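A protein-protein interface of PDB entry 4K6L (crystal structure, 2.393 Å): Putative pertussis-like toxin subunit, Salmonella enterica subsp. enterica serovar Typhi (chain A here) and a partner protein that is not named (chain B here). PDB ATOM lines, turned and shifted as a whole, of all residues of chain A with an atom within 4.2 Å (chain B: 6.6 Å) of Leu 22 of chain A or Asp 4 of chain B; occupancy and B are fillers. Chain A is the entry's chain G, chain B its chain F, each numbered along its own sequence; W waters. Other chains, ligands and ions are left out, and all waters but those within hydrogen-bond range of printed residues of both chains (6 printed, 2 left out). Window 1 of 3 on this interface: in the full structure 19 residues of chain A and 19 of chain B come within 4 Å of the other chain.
Water W3 lies within hydrogen-bond range of OG of Ser 21 of chain A (2.5 Å), OG of Ser 121 of chain A (2.7 Å), OG of Ser 3 of chain B (3.0 Å) and ND2 of Asn 1 of chain B (3.1 Å).
Water W2 lies within hydrogen-bond range of OG of Ser 3 of chain B (2.7 Å), OD1 of Asp 4 of chain B (2.9 Å), OG of Ser 21 of chain A (3.3 Å) and NH1 of Arg 224 of chain B (3.4 Å).
Water W5 lies within hydrogen-bond range of the side-chain carboxylate (OD1) of Asp 38 of chain B and the guanidinium group (NH1) of Arg 46 of chain A.
Water W6 lies within hydrogen-bond range of N of Asn 1 of chain B (2.9 Å) and O of Ser 121 of chain A (3.1 Å).
Water W4 bridges the backbone carbonyl oxygen of Gly 24 of chain A (3.0 Å) and the backbone carbonyl oxygen of Ser 3 of chain B (3.1 Å).
Water W1 lies within hydrogen-bond range of O of Ile 2 of chain B (3.0 Å), O of Tyr 5 of chain B (3.0 Å) and OH of Tyr 25 of chain A (3.2 Å).
O of Ser 3 of chain B is in hydrogen-bond range of OH of Tyr 25 of chain A (3.0 Å).
NH2 of Arg 46 of chain A sits at hydrogen-bond distance from O of Asp 4 of chain B.
OD1 of Asp 4 of chain B lies within hydrogen-bond range of OG of Ser 121 of chain A (2.5 Å).
O of Tyr 5 of chain B sits at hydrogen-bond distance from OH of Tyr 25 of chain A, at 2.9 Å.
NH2 of Arg 46 of chain A lies within salt-bridge range of OD2 of Asp 38 of chain B (2.7 Å).
NH1 of Arg 224 of chain B lies within hydrogen-bond range of OG of Ser 21 of chain A.
The guanidinium group (NH1) of Arg 224 of chain B is in hydrogen-bond range of the backbone carbonyl oxygen (O) of Leu 22 of chain A, 2.6 Å away.
O of Leu 23 of chain A lies within hydrogen-bond range of NH2 of Arg 224 of chain B (3.1 Å).
NE of Arg 224 of chain B sits close to SG of Cys 196 of chain A (3.5 Å).
The backbone NH (N) of Ala 244 of chain B is in hydrogen-bond range of the side-chain hydroxyl (OH) of Tyr 25 of chain A (2.7 Å).
SG of Cys 247 of chain B forms a disulfide with SG of Cys 196 of chain A.
Of the 14 printed residues of chain A, 8 touch a printed residue of chain B.
Hydrophobic or aromatic side chains of chain A that line the printed part of chain B: Leu 22, Leu 23, Tyr 25 and Leu 120.
Of the 13 printed residues of chain B, 10 touch a printed residue of chain A.
Printed residues of chain B that touch a printed residue of chain A: Asn 1, Ser 3, Asp 4, Tyr 5, Lys 6, Asp 38, Tyr 221, Arg 224, Ala 244 and Cys 247.
Hydrophobic or aromatic side chains of chain B that line the printed part of chain A: Tyr 5, Tyr 221 and Ala 244.
Along chain B the printed residues that touch a printed residue of chain A span positions 1 to 247.
Among the printed residues, Asp or Glu carboxylates within 4 Å of a Lys or Arg side-chain nitrogen of the other chain: Arg 46 of chain A with Asp 38 of chain B (2.7 Å).
Of chain B, only Asp 4 and Arg 224 come within 4 Å of Leu 22 of chain A.
Of the printed residues of chain A, Asp 4 of chain B touches Leu 22 (3.3 Å), Tyr 25 (3.8 Å), Arg 46 (3.0 Å), Leu 120 (3.7 Å) and Ser 121 (2.5 Å).
Of the printed residues of chain A, Asp 38 of chain B touches Arg 46 (2.7 Å).
Of the printed residues of chain B, Leu 23 of chain A touches Arg 224 (3.1 Å) and Cys 247 (3.7 Å).
Printed residues of chain A within 4 Å of Ser 3 of chain B: Tyr 25 (3.0 Å).
Printed residues of chain A within 4 Å of Tyr 5 of chain B: Tyr 25 (2.9 Å), Arg 46 (3.8 Å) and Leu 120 (3.7 Å).
Printed residues of chain B within 4 Å of Cys 196 of chain A: Tyr 221 (3.6 Å), Arg 224 (3.4 Å) and Cys 247 (2.0 Å).
Arg 245 of chain B touches none of the printed residues of chain A.
The nearest residue of chain B that does not touch Leu 22 of chain A is Cys 247 of chain B (5.5 Å).
Tyr 221 of chain B touches Ser 21 of chain A (CZ to CB, 3.5 Å).
CD1 of Leu 22 of chain A touches OD1 of Asp 4 of chain B, 3.3 Å away.
Cys 247 of chain B touches Leu 23 of chain A (C to CD2, 3.7 Å).
Tyr 25 of chain A touches Asp 4 of chain B.
Tyr 25 of chain A touches Lys 6 of chain B (CG to CE, 3.6 Å).
Tyr 5 of chain B touches Arg 46 of chain A.
Arg 46 of chain A touches Lys 6 of chain B.
Leu 120 of chain A touches Asp 4 of chain B.
Leu 120 of chain A touches Tyr 5 of chain B.
ND2 of Asn 1 of chain B touches CB of Ser 121 of chain A (3.4 Å).
N of Asn 1 of chain B lies within hydrogen-bond range of OD2 of Asp 4 of chain B.
The side-chain carboxylate (OD2) of Asp 132 of chain B lies within hydrogen-bond range of the backbone NH (N) of Asn 1 of chain B (2.7 Å).
The side-chain carboxylate (OD2) of Asp 38 of chain B sits at hydrogen-bond distance from the backbone NH (N) of Lys 6 of chain B (2.6 Å).
The backbone NH (N) of Leu 23 of chain A sits at hydrogen-bond distance from the backbone carbonyl oxygen (O) of Ser 45 of chain A, at 3.3 Å.
The backbone carbonyl oxygen of Tyr 25 of chain A lies close to the guanidinium group of Arg 46 of chain A (3.5 Å).
OG of Ser 118 of chain A is in hydrogen-bond range of O of Leu 120 of chain A (2.7 Å).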
ATOM      1  N   SER A  21       4.785 -32.088 -19.305  1.00  0.00           N
ATOM      2  CA  SER A  21       5.670 -30.931 -19.168  1.00  0.00           C
ATOM      3  C   SER A  21       5.904 -30.525 -17.706  1.00  0.00           C
ATOM      4  O   SER A  21       5.005 -30.632 -16.870  1.00  0.00           O
ATOM      5  CB  SER A  21       5.105 -29.746 -19.965  1.00  0.00           C
ATOM      6  OG  SER A  21       5.997 -28.649 -19.996  1.00  0.00           O
ATOM      7  N   LEU A  22       7.116 -30.060 -17.405  1.00  0.00           N
ATOM      8  CA  LEU A  22       7.442 -29.559 -16.070  1.00  0.00           C
ATOM      9  C   LEU A  22       6.643 -28.297 -15.777  1.00  0.00           C
ATOM     10  O   LEU A  22       6.291 -27.557 -16.687  1.00  0.00           O
ATOM     11  CB  LEU A  22       8.929 -29.222 -15.960  1.00  0.00           C
ATOM     12  CG  LEU A  22       9.939 -30.304 -16.328  1.00  0.00           C
ATOM     13  CD1 LEU A  22      11.360 -29.747 -16.255  1.00  0.00           C
ATOM     14  CD2 LEU A  22       9.784 -31.496 -15.416  1.00  0.00           C
ATOM     15  N   LEU A  23       6.372 -28.050 -14.502  1.00  0.00           N
ATOM     16  CA  LEU A  23       5.694 -26.828 -14.089  1.00  0.00           C
ATOM     17  C   LEU A  23       6.589 -25.596 -14.262  1.00  0.00           C
ATOM     18  O   LEU A  23       6.140 -24.569 -14.766  1.00  0.00           O
ATOM     19  CB  LEU A  23       5.205 -26.939 -12.640  1.00  0.00           C
ATOM     20  CG  LEU A  23       3.946 -27.787 -12.428  1.00  0.00           C
ATOM     21  CD1 LEU A  23       3.556 -27.828 -10.964  1.00  0.00           C
ATOM     22  CD2 LEU A  23       2.802 -27.224 -13.270  1.00  0.00           C
ATOM     23  N   GLY A  24       7.850 -25.701 -13.848  1.00  0.00           N
ATOM     24  CA  GLY A  24       8.761 -24.577 -13.960  1.00  0.00           C
ATOM     25  C   GLY A  24      10.222 -24.929 -13.762  1.00  0.00           C
ATOM     26  O   GLY A  24      10.655 -26.022 -14.130  1.00  0.00           O
ATOM     27  N   TYR A  25      10.972 -23.999 -13.166  1.00  0.00           N
ATOM     28  CA  TYR A  25      12.421 -24.130 -13.007  1.00  0.00           C
ATOM     29  C   TYR A  25      12.890 -24.315 -11.548  1.00  0.00           C
ATOM     30  O   TYR A  25      14.090 -24.292 -11.264  1.00  0.00           O
ATOM     31  CB  TYR A  25      13.131 -22.909 -13.608  1.00  0.00           C
ATOM     32  CG  TYR A  25      12.935 -22.706 -15.102  1.00  0.00           C
ATOM     33  CD1 TYR A  25      13.372 -23.656 -16.020  1.00  0.00           C
ATOM     34  CD2 TYR A  25      12.345 -21.545 -15.593  1.00  0.00           C
ATOM     35  CE1 TYR A  25      13.206 -23.469 -17.381  1.00  0.00           C
ATOM     36  CE2 TYR A  25      12.174 -21.345 -16.957  1.00  0.00           C
ATOM     37  CZ  TYR A  25      12.608 -22.310 -17.846  1.00  0.00           C
ATOM     38  OH  TYR A  25      12.447 -22.117 -19.202  1.00  0.00           O
ATOM     39  N   SER A  45       7.640 -26.401  -9.904  1.00  0.00           N
ATOM     40  CA  SER A  45       8.600 -27.494  -9.765  1.00  0.00           C
ATOM     41  C   SER A  45       9.250 -27.887 -11.090  1.00  0.00           C
ATOM     42  O   SER A  45       8.579 -27.994 -12.116  1.00  0.00           O
ATOM     43  CB  SER A  45       7.922 -28.717  -9.151  1.00  0.00           C
ATOM     44  OG  SER A  45       6.862 -29.165  -9.975  1.00  0.00           O
ATOM     45  N   ARG A  46      10.563 -28.110 -11.046  1.00  0.00           N
ATOM     46  CA  ARG A  46      11.337 -28.537 -12.206  1.00  0.00           C
ATOM     47  C   ARG A  46      11.490 -30.055 -12.213  1.00  0.00           C
ATOM     48  O   ARG A  46      12.510 -30.588 -12.652  1.00  0.00           O
ATOM     49  CB  ARG A  46      12.716 -27.882 -12.171  1.00  0.00           C
ATOM     50  CG  ARG A  46      13.432 -27.808 -13.508  1.00  0.00           C
ATOM     51  CD  ARG A  46      14.671 -26.958 -13.356  1.00  0.00           C
ATOM     52  NE  ARG A  46      15.312 -26.681 -14.631  1.00  0.00           N
ATOM     53  CZ  ARG A  46      16.094 -25.632 -14.849  1.00  0.00           C
ATOM     54  NH1 ARG A  46      16.322 -24.757 -13.875  1.00  0.00           N
ATOM     55  NH2 ARG A  46      16.636 -25.450 -16.047  1.00  0.00           N
ATOM     56  N   TYR A  47      10.479 -30.747 -11.696  1.00  0.00           N
ATOM     57  CA  TYR A  47      10.459 -32.204 -11.719  1.00  0.00           C
ATOM     58  C   TYR A  47       9.053 -32.700 -12.026  1.00  0.00           C
ATOM     59  O   TYR A  47       8.072 -31.995 -11.807  1.00  0.00           O
ATOM     60  CB  TYR A  47      10.907 -32.787 -10.371  1.00  0.00           C
ATOM     61  CG  TYR A  47      12.222 -32.253  -9.832  1.00  0.00           C
ATOM     62  CD1 TYR A  47      13.443 -32.728 -10.311  1.00  0.00           C
ATOM     63  CD2 TYR A  47      12.242 -31.291  -8.822  1.00  0.00           C
ATOM     64  CE1 TYR A  47      14.644 -32.249  -9.809  1.00  0.00           C
ATOM     65  CE2 TYR A  47      13.437 -30.807  -8.316  1.00  0.00           C
ATOM     66  CZ  TYR A  47      14.635 -31.288  -8.812  1.00  0.00           C
ATOM     67  OH  TYR A  47      15.825 -30.803  -8.309  1.00  0.00           O
ATOM     68  N   ILE A  48       8.960 -33.921 -12.537  1.00  0.00           N
ATOM     69  CA  ILE A  48       7.678 -34.601 -12.632  1.00  0.00           C
ATOM     70  C   ILE A  48       7.730 -35.856 -11.774  1.00  0.00           C
ATOM     71  O   ILE A  48       8.637 -36.681 -11.907  1.00  0.00           O
ATOM     72  CB  ILE A  48       7.318 -34.975 -14.077  1.00  0.00           C
ATOM     73  CG1 ILE A  48       7.062 -33.710 -14.899  1.00  0.00           C
ATOM     74  CG2 ILE A  48       6.087 -35.861 -14.097  1.00  0.00           C
ATOM     75  CD1 ILE A  48       7.068 -33.932 -16.402  1.00  0.00           C
ATOM     76  N   SER A 118      11.348 -37.176 -12.703  1.00  0.00           N
ATOM     77  CA  SER A 118      11.977 -36.884 -13.982  1.00  0.00           C
ATOM     78  C   SER A 118      12.468 -35.446 -13.983  1.00  0.00           C
ATOM     79  O   SER A 118      11.718 -34.530 -13.635  1.00  0.00           O
ATOM     80  CB  SER A 118      10.994 -37.110 -15.128  1.00  0.00           C
ATOM     81  OG  SER A 118      11.582 -36.773 -16.372  1.00  0.00           O
ATOM     82  N   THR A 119      13.726 -35.253 -14.371  1.00  0.00           N
ATOM     83  CA  THR A 119      14.332 -33.927 -14.371  1.00  0.00           C
ATOM     84  C   THR A 119      14.012 -33.137 -15.635  1.00  0.00           C
ATOM     85  O   THR A 119      14.167 -31.915 -15.675  1.00  0.00           O
ATOM     86  CB  THR A 119      15.863 -34.002 -14.191  1.00  0.00           C
ATOM     87  OG1 THR A 119      16.427 -34.848 -15.201  1.00  0.00           O
ATOM     88  CG2 THR A 119      16.202 -34.554 -12.822  1.00  0.00           C
ATOM     89  N   LEU A 120      13.574 -33.848 -16.666  1.00  0.00           N
ATOM     90  CA  LEU A 120      13.179 -33.227 -17.923  1.00  0.00           C
ATOM     91  C   LEU A 120      11.716 -33.531 -18.177  1.00  0.00           C
ATOM     92  O   LEU A 120      11.116 -34.342 -17.470  1.00  0.00           O
ATOM     93  CB  LEU A 120      14.017 -33.782 -19.075  1.00  0.00           C
ATOM     94  CG  LEU A 120      15.521 -33.523 -19.023  1.00  0.00           C
ATOM     95  CD1 LEU A 120      16.198 -34.187 -20.209  1.00  0.00           C
ATOM     96  CD2 LEU A 120      15.810 -32.022 -18.990  1.00  0.00           C
ATOM     97  N   SER A 121      11.140 -32.888 -19.189  1.00  0.00           N
ATOM     98  CA  SER A 121       9.788 -33.226 -19.616  1.00  0.00           C
ATOM     99  C   SER A 121       9.773 -34.671 -20.092  1.00  0.00           C
ATOM    100  O   SER A 121      10.804 -35.210 -20.505  1.00  0.00           O
ATOM    101  CB  SER A 121       9.317 -32.301 -20.742  1.00  0.00           C
ATOM    102  OG  SER A 121       9.240 -30.958 -20.306  1.00  0.00           O
ATOM    103  N   CYS A 196       2.319 -29.423 -16.389  1.00  0.00           N
ATOM    104  CA  CYS A 196       1.736 -28.268 -17.072  1.00  0.00           C
ATOM    105  C   CYS A 196       0.792 -28.710 -18.186  1.00  0.00           C
ATOM    106  O   CYS A 196       1.215 -29.338 -19.155  1.00  0.00           O
ATOM    107  CB  CYS A 196       2.833 -27.351 -17.629  1.00  0.00           C
ATOM    108  SG  CYS A 196       2.253 -25.741 -18.241  1.00  0.00           S
ATOM    109  N   ASN B   1      12.760 -31.291 -23.448  1.00  0.00           N
ATOM    110  CA  ASN B   1      12.106 -30.209 -24.179  1.00  0.00           C
ATOM    111  C   ASN B   1      12.816 -28.873 -23.990  1.00  0.00           C
ATOM    112  O   ASN B   1      13.580 -28.693 -23.040  1.00  0.00           O
ATOM    113  CB  ASN B   1      10.629 -30.096 -23.784  1.00  0.00           C
ATOM    114  CG  ASN B   1       9.833 -31.337 -24.141  1.00  0.00           C
ATOM    115  OD1 ASN B   1      10.389 -32.320 -24.630  1.00  0.00           O
ATOM    116  ND2 ASN B   1       8.528 -31.305 -23.882  1.00  0.00           N
ATOM    117  N   ILE B   2      12.556 -27.936 -24.897  1.00  0.00           N
ATOM    118  CA  ILE B   2      13.207 -26.630 -24.858  1.00  0.00           C
ATOM    119  C   ILE B   2      12.854 -25.843 -23.588  1.00  0.00           C
ATOM    120  O   ILE B   2      13.694 -25.127 -23.029  1.00  0.00           O
ATOM    121  CB  ILE B   2      12.857 -25.807 -26.117  1.00  0.00           C
ATOM    122  CG1 ILE B   2      13.146 -26.628 -27.379  1.00  0.00           C
ATOM    123  CG2 ILE B   2      13.619 -24.493 -26.141  1.00  0.00           C
ATOM    124  CD1 ILE B   2      14.590 -27.087 -27.504  1.00  0.00           C
ATOM    125  N   SER B   3      11.614 -25.990 -23.127  1.00  0.00           N
ATOM    126  CA  SER B   3      11.141 -25.244 -21.963  1.00  0.00           C
ATOM    127  C   SER B   3      11.767 -25.715 -20.643  1.00  0.00           C
ATOM    128  O   SER B   3      11.665 -25.025 -19.630  1.00  0.00           O
ATOM    129  CB  SER B   3       9.616 -25.310 -21.867  1.00  0.00           C
ATOM    130  OG  SER B   3       9.185 -26.646 -21.670  1.00  0.00           O
ATOM    131  N   ASP B   4      12.409 -26.882 -20.658  1.00  0.00           N
ATOM    132  CA  ASP B   4      13.038 -27.437 -19.453  1.00  0.00           C
ATOM    133  C   ASP B   4      14.316 -26.692 -19.061  1.00  0.00           C
ATOM    134  O   ASP B   4      14.810 -26.824 -17.939  1.00  0.00           O
ATOM    135  CB  ASP B   4      13.362 -28.921 -19.651  1.00  0.00           C
ATOM    136  CG  ASP B   4      12.126 -29.761 -19.925  1.00  0.00           C
ATOM    137  OD1 ASP B   4      11.022 -29.386 -19.473  1.00  0.00           O
ATOM    138  OD2 ASP B   4      12.264 -30.807 -20.591  1.00  0.00           O
ATOM    139  N   TYR B   5      14.847 -25.916 -19.997  1.00  0.00           N
ATOM    140  CA  TYR B   5      16.104 -25.209 -19.802  1.00  0.00           C
ATOM    141  C   TYR B   5      15.865 -23.707 -19.731  1.00  0.00           C
ATOM    142  O   TYR B   5      14.884 -23.197 -20.272  1.00  0.00           O
ATOM    143  CB  TYR B   5      17.054 -25.516 -20.963  1.00  0.00           C
ATOM    144  CG  TYR B   5      17.406 -26.982 -21.099  1.00  0.00           C
ATOM    145  CD1 TYR B   5      16.551 -27.865 -21.746  1.00  0.00           C
ATOM    146  CD2 TYR B   5      18.593 -27.483 -20.579  1.00  0.00           C
ATOM    147  CE1 TYR B   5      16.868 -29.205 -21.870  1.00  0.00           C
ATOM    148  CE2 TYR B   5      18.916 -28.824 -20.699  1.00  0.00           C
ATOM    149  CZ  TYR B   5      18.049 -29.678 -21.345  1.00  0.00           C
ATOM    150  OH  TYR B   5      18.369 -31.010 -21.462  1.00  0.00           O
ATOM    151  N   LYS B   6      16.754 -22.997 -19.051  1.00  0.00           N
ATOM    152  CA  LYS B   6      16.773 -21.549 -19.161  1.00  0.00           C
ATOM    153  C   LYS B   6      17.750 -21.218 -20.274  1.00  0.00           C
ATOM    154  O   LYS B   6      18.953 -21.427 -20.140  1.00  0.00           O
ATOM    155  CB  LYS B   6      17.194 -20.889 -17.848  1.00  0.00           C
ATOM    156  CG  LYS B   6      16.164 -21.009 -16.732  1.00  0.00           C
ATOM    157  CD  LYS B   6      16.594 -20.232 -15.494  1.00  0.00           C
ATOM    158  CE  LYS B   6      15.598 -20.412 -14.369  1.00  0.00           C
ATOM    159  NZ  LYS B   6      15.913 -19.564 -13.188  1.00  0.00           N
ATOM    160  N   ASP B  38      21.038 -22.021 -18.201  1.00  0.00           N
ATOM    161  CA  ASP B  38      21.588 -23.342 -18.504  1.00  0.00           C
ATOM    162  C   ASP B  38      22.266 -23.385 -19.861  1.00  0.00           C
ATOM    163  O   ASP B  38      23.343 -23.957 -20.000  1.00  0.00           O
ATOM    164  CB  ASP B  38      20.496 -24.405 -18.441  1.00  0.00           C
ATOM    165  CG  ASP B  38      19.674 -24.300 -17.187  1.00  0.00           C
ATOM    166  OD1 ASP B  38      20.218 -24.591 -16.102  1.00  0.00           O
ATOM    167  OD2 ASP B  38      18.489 -23.915 -17.285  1.00  0.00           O
ATOM    168  N   ASP B 132      16.949 -32.729 -27.296  1.00  0.00           N
ATOM    169  CA  ASP B 132      16.896 -31.293 -27.530  1.00  0.00           C
ATOM    170  C   ASP B 132      18.179 -30.796 -28.167  1.00  0.00           C
ATOM    171  O   ASP B 132      19.269 -31.271 -27.831  1.00  0.00           O
ATOM    172  CB  ASP B 132      16.641 -30.555 -26.215  1.00  0.00           C
ATOM    173  CG  ASP B 132      15.341 -30.978 -25.562  1.00  0.00           C
ATOM    174  OD1 ASP B 132      14.312 -30.999 -26.265  1.00  0.00           O
ATOM    175  OD2 ASP B 132      15.348 -31.318 -24.360  1.00  0.00           O
ATOM    176  N   TYR B 221       5.422 -28.611 -26.458  1.00  0.00           N
ATOM    177  CA  TYR B 221       5.352 -27.461 -25.555  1.00  0.00           C
ATOM    178  C   TYR B 221       6.198 -26.267 -26.016  1.00  0.00           C
ATOM    179  O   TYR B 221       6.656 -25.461 -25.203  1.00  0.00           O
ATOM    180  CB  TYR B 221       5.688 -27.871 -24.114  1.00  0.00           C
ATOM    181  CG  TYR B 221       4.737 -28.910 -23.558  1.00  0.00           C
ATOM    182  CD1 TYR B 221       3.523 -28.539 -22.986  1.00  0.00           C
ATOM    183  CD2 TYR B 221       5.045 -30.268 -23.618  1.00  0.00           C
ATOM    184  CE1 TYR B 221       2.644 -29.487 -22.490  1.00  0.00           C
ATOM    185  CE2 TYR B 221       4.175 -31.223 -23.121  1.00  0.00           C
ATOM    186  CZ  TYR B 221       2.976 -30.831 -22.558  1.00  0.00           C
ATOM    187  OH  TYR B 221       2.113 -31.787 -22.059  1.00  0.00           O
ATOM    188  N   ARG B 224       5.304 -22.647 -24.976  1.00  0.00           N
ATOM    189  CA  ARG B 224       5.577 -22.177 -23.622  1.00  0.00           C
ATOM    190  C   ARG B 224       6.787 -21.257 -23.589  1.00  0.00           C
ATOM    191  O   ARG B 224       6.933 -20.444 -22.683  1.00  0.00           O
ATOM    192  CB  ARG B 224       5.804 -23.352 -22.672  1.00  0.00           C
ATOM    193  CG  ARG B 224       4.573 -24.198 -22.427  1.00  0.00           C
ATOM    194  CD  ARG B 224       4.779 -25.105 -21.236  1.00  0.00           C
ATOM    195  NE  ARG B 224       4.974 -24.336 -20.013  1.00  0.00           N
ATOM    196  CZ  ARG B 224       5.455 -24.849 -18.885  1.00  0.00           C
ATOM    197  NH1 ARG B 224       5.789 -26.130 -18.838  1.00  0.00           N
ATOM    198  NH2 ARG B 224       5.593 -24.084 -17.808  1.00  0.00           N
ATOM    199  N   ALA B 244      10.285 -20.699 -19.998  1.00  0.00           N
ATOM    200  CA  ALA B 244       8.939 -21.236 -20.000  1.00  0.00           C
ATOM    201  C   ALA B 244       8.042 -20.305 -19.197  1.00  0.00           C
ATOM    202  O   ALA B 244       8.410 -19.870 -18.105  1.00  0.00           O
ATOM    203  CB  ALA B 244       8.919 -22.637 -19.412  1.00  0.00           C
ATOM    204  N   ARG B 245       6.877 -19.988 -19.754  1.00  0.00           N
ATOM    205  CA  ARG B 245       5.881 -19.194 -19.053  1.00  0.00           C
ATOM    206  C   ARG B 245       5.415 -19.955 -17.826  1.00  0.00           C
ATOM    207  O   ARG B 245       5.493 -21.173 -17.791  1.00  0.00           O
ATOM    208  CB  ARG B 245       4.677 -18.919 -19.952  1.00  0.00           C
ATOM    209  CG  ARG B 245       4.981 -18.112 -21.194  1.00  0.00           C
ATOM    210  CD  ARG B 245       3.726 -17.395 -21.660  1.00  0.00           C
ATOM    211  NE  ARG B 245       3.914 -16.758 -22.957  1.00  0.00           N
ATOM    212  CZ  ARG B 245       3.704 -17.370 -24.115  1.00  0.00           C
ATOM    213  NH1 ARG B 245       3.298 -18.631 -24.128  1.00  0.00           N
ATOM    214  NH2 ARG B 245       3.900 -16.722 -25.257  1.00  0.00           N
ATOM    215  N   CYS B 247       3.114 -21.780 -15.006  1.00  0.00           N
ATOM    216  CA  CYS B 247       2.095 -22.804 -15.191  1.00  0.00           C
ATOM    217  C   CYS B 247       1.972 -23.695 -13.964  1.00  0.00           C
ATOM    218  O   CYS B 247       1.609 -23.237 -12.885  1.00  0.00           O
ATOM    219  CB  CYS B 247       2.421 -23.674 -16.403  1.00  0.00           C
ATOM    220  SG  CYS B 247       1.271 -25.041 -16.611  1.00  0.00           S
HETATM  221  O   HOH W   1      12.943 -22.292 -22.408  1.00  0.00           O
HETATM  222  O   HOH W   2       8.935 -27.475 -19.106  1.00  0.00           O
HETATM  223  O   HOH W   3       7.644 -29.237 -21.732  1.00  0.00           O
HETATM  224  O   HOH W   4      10.130 -25.752 -17.054  1.00  0.00           O
HETATM  225  O   HOH W   5      18.655 -23.228 -14.276  1.00  0.00           O
HETATM  226  O   HOH W   6      12.628 -34.095 -22.743  1.00  0.00           O
